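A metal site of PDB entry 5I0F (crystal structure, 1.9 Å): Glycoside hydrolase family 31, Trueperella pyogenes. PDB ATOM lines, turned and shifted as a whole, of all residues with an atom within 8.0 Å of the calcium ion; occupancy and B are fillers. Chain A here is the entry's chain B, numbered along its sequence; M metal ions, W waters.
The calcium ion is bound by the backbone carbonyl oxygen (O) of Leu 254, water W3, water W2, water W1, the side-chain carboxylate (OD1) of Asp 253, the side-chain carboxylate (OD2) of Asp 253 and the side-chain carboxylate (OD2) of Asp 486. The calcium ion has seven donor atoms within binding distance.
The backbone NH of Leu 254 lies within hydrogen-bond range of the backbone carbonyl oxygen of His 161, 2.9 Å away. N of Asp 253 lies within hydrogen-bond range of O of Arg 235. OD2 of Asp 486 sits close to NE of Arg 234 (3.1 Å). The backbone NH (N) of Asp 486 is in hydrogen-bond range of the backbone carbonyl oxygen (O) of Ser 475 (3.0 Å).
O of Gly 255 touches the calcium ion (3.7 Å).
Water W1 lies within hydrogen-bond range of O of His 161 (3.1 Å) and O of Gly 255 (3.1 Å).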
ATOM      1  N   ARG A   7      -6.206  -7.622  22.353  1.00  0.00           N
ATOM      2  CA  ARG A   7      -7.485  -7.978  21.698  1.00  0.00           C
ATOM      3  C   ARG A   7      -7.316  -8.603  20.326  1.00  0.00           C
ATOM      4  O   ARG A   7      -8.309  -9.029  19.718  1.00  0.00           O
ATOM      5  CB  ARG A   7      -8.391  -6.752  21.612  1.00  0.00           C
ATOM      6  CG  ARG A   7      -8.932  -6.290  22.957  1.00  0.00           C
ATOM      7  CD  ARG A   7      -9.686  -4.962  22.812  1.00  0.00           C
ATOM      8  NE  ARG A   7      -8.771  -3.874  23.116  1.00  0.00           N
ATOM      9  CZ  ARG A   7      -8.165  -3.065  22.252  1.00  0.00           C
ATOM     10  NH1 ARG A   7      -8.375  -3.134  20.954  1.00  0.00           N
ATOM     11  NH2 ARG A   7      -7.338  -2.142  22.718  1.00  0.00           N
ATOM     12  N   ILE A  24     -10.724 -10.024  27.487  1.00  0.00           N
ATOM     13  CA  ILE A  24     -10.918  -9.397  28.815  1.00  0.00           C
ATOM     14  C   ILE A  24     -10.743 -10.529  29.845  1.00  0.00           C
ATOM     15  O   ILE A  24     -11.660 -11.344  30.043  1.00  0.00           O
ATOM     16  CB  ILE A  24     -12.344  -8.770  28.957  1.00  0.00           C
ATOM     17  CG1 ILE A  24     -12.573  -7.682  27.883  1.00  0.00           C
ATOM     18  CG2 ILE A  24     -12.585  -8.236  30.370  1.00  0.00           C
ATOM     19  CD1 ILE A  24     -11.625  -6.498  27.952  1.00  0.00           C
ATOM     20  N   THR A 160     -15.700  -1.118  34.294  1.00  0.00           N
ATOM     21  CA  THR A 160     -16.821  -2.046  34.099  1.00  0.00           C
ATOM     22  C   THR A 160     -16.954  -2.354  32.613  1.00  0.00           C
ATOM     23  O   THR A 160     -17.157  -1.437  31.806  1.00  0.00           O
ATOM     24  CB  THR A 160     -18.129  -1.424  34.655  1.00  0.00           C
ATOM     25  OG1 THR A 160     -17.887  -0.976  35.982  1.00  0.00           O
ATOM     26  CG2 THR A 160     -19.263  -2.437  34.672  1.00  0.00           C
ATOM     27  N   HIS A 161     -16.819  -3.616  32.248  1.00  0.00           N
ATOM     28  CA  HIS A 161     -16.615  -3.986  30.842  1.00  0.00           C
ATOM     29  C   HIS A 161     -17.851  -4.521  30.137  1.00  0.00           C
ATOM     30  O   HIS A 161     -18.034  -4.270  28.939  1.00  0.00           O
ATOM     31  CB  HIS A 161     -15.482  -4.997  30.720  1.00  0.00           C
ATOM     32  CG  HIS A 161     -14.246  -4.571  31.442  1.00  0.00           C
ATOM     33  ND1 HIS A 161     -13.399  -3.607  30.960  1.00  0.00           N
ATOM     34  CD2 HIS A 161     -13.737  -4.948  32.638  1.00  0.00           C
ATOM     35  CE1 HIS A 161     -12.411  -3.415  31.811  1.00  0.00           C
ATOM     36  NE2 HIS A 161     -12.593  -4.216  32.851  1.00  0.00           N
ATOM     37  N   ARG A 162     -18.654  -5.291  30.865  1.00  0.00           N
ATOM     38  CA  ARG A 162     -19.874  -5.928  30.334  1.00  0.00           C
ATOM     39  C   ARG A 162     -20.934  -6.015  31.425  1.00  0.00           C
ATOM     40  O   ARG A 162     -20.632  -5.904  32.620  1.00  0.00           O
ATOM     41  CB  ARG A 162     -19.590  -7.338  29.801  1.00  0.00           C
ATOM     42  CG  ARG A 162     -18.662  -7.378  28.586  1.00  0.00           C
ATOM     43  CD  ARG A 162     -18.941  -8.557  27.666  1.00  0.00           C
ATOM     44  NE  ARG A 162     -18.656  -9.819  28.330  1.00  0.00           N
ATOM     45  CZ  ARG A 162     -17.443 -10.368  28.451  1.00  0.00           C
ATOM     46  NH1 ARG A 162     -16.357  -9.769  27.974  1.00  0.00           N
ATOM     47  NH2 ARG A 162     -17.313 -11.524  29.071  1.00  0.00           N
ATOM     48  N   ARG A 234     -23.146  -1.117  20.534  1.00  0.00           N
ATOM     49  CA  ARG A 234     -22.126  -2.075  20.924  1.00  0.00           C
ATOM     50  C   ARG A 234     -22.687  -3.478  20.753  1.00  0.00           C
ATOM     51  O   ARG A 234     -23.877  -3.678  20.568  1.00  0.00           O
ATOM     52  CB  ARG A 234     -21.665  -1.851  22.375  1.00  0.00           C
ATOM     53  CG  ARG A 234     -21.151  -0.450  22.628  1.00  0.00           C
ATOM     54  CD  ARG A 234     -20.337  -0.343  23.922  1.00  0.00           C
ATOM     55  NE  ARG A 234     -19.840   1.009  24.175  1.00  0.00           N
ATOM     56  CZ  ARG A 234     -20.515   2.013  24.744  1.00  0.00           C
ATOM     57  NH1 ARG A 234     -21.796   1.884  25.126  1.00  0.00           N
ATOM     58  NH2 ARG A 234     -19.915   3.197  24.923  1.00  0.00           N
ATOM     59  N   ARG A 235     -21.787  -4.454  20.812  1.00  0.00           N
ATOM     60  CA  ARG A 235     -22.155  -5.848  20.622  1.00  0.00           C
ATOM     61  C   ARG A 235     -23.023  -6.332  21.780  1.00  0.00           C
ATOM     62  O   ARG A 235     -22.825  -5.914  22.928  1.00  0.00           O
ATOM     63  CB  ARG A 235     -20.901  -6.686  20.525  1.00  0.00           C
ATOM     64  CG  ARG A 235     -21.130  -8.127  20.153  1.00  0.00           C
ATOM     65  CD  ARG A 235     -19.812  -8.733  19.758  1.00  0.00           C
ATOM     66  NE  ARG A 235     -19.920 -10.111  19.280  1.00  0.00           N
ATOM     67  CZ  ARG A 235     -18.855 -10.840  18.922  1.00  0.00           C
ATOM     68  NH1 ARG A 235     -19.010 -12.075  18.484  1.00  0.00           N
ATOM     69  NH2 ARG A 235     -17.625 -10.332  19.046  1.00  0.00           N
ATOM     70  N   VAL A 252     -24.255  -7.465  27.337  1.00  0.00           N
ATOM     71  CA  VAL A 252     -24.062  -6.221  26.630  1.00  0.00           C
ATOM     72  C   VAL A 252     -22.630  -5.748  26.856  1.00  0.00           C
ATOM     73  O   VAL A 252     -22.160  -5.662  28.014  1.00  0.00           O
ATOM     74  CB  VAL A 252     -25.045  -5.158  27.175  1.00  0.00           C
ATOM     75  CG1 VAL A 252     -24.903  -3.855  26.428  1.00  0.00           C
ATOM     76  CG2 VAL A 252     -26.480  -5.666  27.147  1.00  0.00           C
ATOM     77  N   ASP A 253     -21.930  -5.457  25.767  1.00  0.00           N
ATOM     78  CA  ASP A 253     -20.614  -4.789  25.859  1.00  0.00           C
ATOM     79  C   ASP A 253     -20.819  -3.344  26.316  1.00  0.00           C
ATOM     80  O   ASP A 253     -21.760  -2.668  25.871  1.00  0.00           O
ATOM     81  CB  ASP A 253     -19.884  -4.857  24.516  1.00  0.00           C
ATOM     82  CG  ASP A 253     -18.585  -4.092  24.504  1.00  0.00           C
ATOM     83  OD1 ASP A 253     -17.784  -4.233  25.453  1.00  0.00           O
ATOM     84  OD2 ASP A 253     -18.338  -3.318  23.541  1.00  0.00           O
ATOM     85  N   LEU A 254     -19.955  -2.874  27.218  1.00  0.00           N
ATOM     86  CA  LEU A 254     -19.997  -1.507  27.727  1.00  0.00           C
ATOM     87  C   LEU A 254     -18.827  -0.668  27.207  1.00  0.00           C
ATOM     88  O   LEU A 254     -18.013  -1.172  26.460  1.00  0.00           O
ATOM     89  CB  LEU A 254     -20.019  -1.525  29.252  1.00  0.00           C
ATOM     90  CG  LEU A 254     -21.256  -2.220  29.866  1.00  0.00           C
ATOM     91  CD1 LEU A 254     -21.108  -2.293  31.374  1.00  0.00           C
ATOM     92  CD2 LEU A 254     -22.537  -1.510  29.469  1.00  0.00           C
ATOM     93  N   GLY A 255     -18.769   0.617  27.585  1.00  0.00           N
ATOM     94  CA  GLY A 255     -17.729   1.578  27.114  1.00  0.00           C
ATOM     95  C   GLY A 255     -16.259   1.280  27.415  1.00  0.00           C
ATOM     96  O   GLY A 255     -15.905   0.176  27.845  1.00  0.00           O
ATOM     97  N   PHE A 256     -15.393   2.263  27.160  1.00  0.00           N
ATOM     98  CA  PHE A 256     -13.922   2.085  27.267  1.00  0.00           C
ATOM     99  C   PHE A 256     -13.340   2.990  28.355  1.00  0.00           C
ATOM    100  O   PHE A 256     -13.838   3.010  29.484  1.00  0.00           O
ATOM    101  CB  PHE A 256     -13.257   2.409  25.919  1.00  0.00           C
ATOM    102  CG  PHE A 256     -12.097   1.491  25.558  1.00  0.00           C
ATOM    103  CD1 PHE A 256     -11.121   1.129  26.495  1.00  0.00           C
ATOM    104  CD2 PHE A 256     -11.975   1.015  24.242  1.00  0.00           C
ATOM    105  CE1 PHE A 256     -10.060   0.297  26.133  1.00  0.00           C
ATOM    106  CE2 PHE A 256     -10.906   0.187  23.884  1.00  0.00           C
ATOM    107  CZ  PHE A 256      -9.959  -0.171  24.827  1.00  0.00           C
ATOM    108  N   SER A 475     -12.037  -2.252  18.700  1.00  0.00           N
ATOM    109  CA  SER A 475     -12.856  -1.568  19.682  1.00  0.00           C
ATOM    110  C   SER A 475     -12.387  -0.122  19.937  1.00  0.00           C
ATOM    111  O   SER A 475     -13.180   0.707  20.370  1.00  0.00           O
ATOM    112  CB  SER A 475     -12.862  -2.358  21.005  1.00  0.00           C
ATOM    113  OG  SER A 475     -11.584  -2.245  21.628  1.00  0.00           O
ATOM    114  N   ASP A 476     -11.115   0.169  19.642  1.00  0.00           N
ATOM    115  CA  ASP A 476     -10.478   1.463  19.952  1.00  0.00           C
ATOM    116  C   ASP A 476     -10.261   2.355  18.723  1.00  0.00           C
ATOM    117  O   ASP A 476      -9.585   3.379  18.826  1.00  0.00           O
ATOM    118  CB  ASP A 476      -9.172   1.277  20.725  1.00  0.00           C
ATOM    119  CG  ASP A 476      -8.288   0.156  20.160  1.00  0.00           C
ATOM    120  OD1 ASP A 476      -8.662  -0.561  19.171  1.00  0.00           O
ATOM    121  OD2 ASP A 476      -7.204  -0.050  20.778  1.00  0.00           O
ATOM    122  N   ARG A 484     -15.911   5.579  19.649  1.00  0.00           N
ATOM    123  CA  ARG A 484     -14.844   4.625  19.408  1.00  0.00           C
ATOM    124  C   ARG A 484     -15.430   3.481  18.608  1.00  0.00           C
ATOM    125  O   ARG A 484     -16.652   3.407  18.407  1.00  0.00           O
ATOM    126  CB  ARG A 484     -14.227   4.110  20.711  1.00  0.00           C
ATOM    127  CG  ARG A 484     -13.670   5.180  21.637  1.00  0.00           C
ATOM    128  CD  ARG A 484     -12.791   6.199  20.955  1.00  0.00           C
ATOM    129  NE  ARG A 484     -11.466   5.694  20.602  1.00  0.00           N
ATOM    130  CZ  ARG A 484     -10.424   5.589  21.429  1.00  0.00           C
ATOM    131  NH1 ARG A 484      -9.253   5.128  20.968  1.00  0.00           N
ATOM    132  NH2 ARG A 484     -10.523   5.923  22.724  1.00  0.00           N
ATOM    133  N   GLY A 485     -14.579   2.578  18.171  1.00  0.00           N
ATOM    134  CA  GLY A 485     -15.028   1.491  17.305  1.00  0.00           C
ATOM    135  C   GLY A 485     -16.041   0.571  17.933  1.00  0.00           C
ATOM    136  O   GLY A 485     -16.929   0.049  17.236  1.00  0.00           O
ATOM    137  N   ASP A 486     -15.936   0.364  19.232  1.00  0.00           N
ATOM    138  CA  ASP A 486     -16.903  -0.492  19.903  1.00  0.00           C
ATOM    139  C   ASP A 486     -18.352  -0.030  19.762  1.00  0.00           C
ATOM    140  O   ASP A 486     -19.250  -0.871  19.840  1.00  0.00           O
ATOM    141  CB  ASP A 486     -16.524  -0.721  21.360  1.00  0.00           C
ATOM    142  CG  ASP A 486     -16.663   0.510  22.218  1.00  0.00           C
ATOM    143  OD1 ASP A 486     -16.497   1.649  21.717  1.00  0.00           O
ATOM    144  OD2 ASP A 486     -16.901   0.318  23.418  1.00  0.00           O
ATOM    145  N   GLU A 487     -18.567   1.261  19.506  1.00  0.00           N
ATOM    146  CA  GLU A 487     -19.891   1.790  19.103  1.00  0.00           C
ATOM    147  C   GLU A 487     -20.033   2.074  17.621  1.00  0.00           C
ATOM    148  O   GLU A 487     -21.084   1.874  17.052  1.00  0.00           O
ATOM    149  CB  GLU A 487     -20.184   3.107  19.844  1.00  0.00           C
ATOM    150  CG  GLU A 487     -20.502   2.961  21.293  1.00  0.00           C
ATOM    151  CD  GLU A 487     -21.013   4.276  21.902  1.00  0.00           C
ATOM    152  OE1 GLU A 487     -20.221   5.226  22.032  1.00  0.00           O
ATOM    153  OE2 GLU A 487     -22.213   4.351  22.231  1.00  0.00           O
HETATM  154 CA    CA M   1     -16.543  -1.995  24.910  1.00  0.00          CA
HETATM  155  O   HOH W   1     -15.938  -2.875  27.215  1.00  0.00           O
HETATM  156  O   HOH W   2     -14.649  -0.433  25.199  1.00  0.00           O
HETATM  157  O   HOH W   3     -15.262  -3.398  23.557  1.00  0.00           O
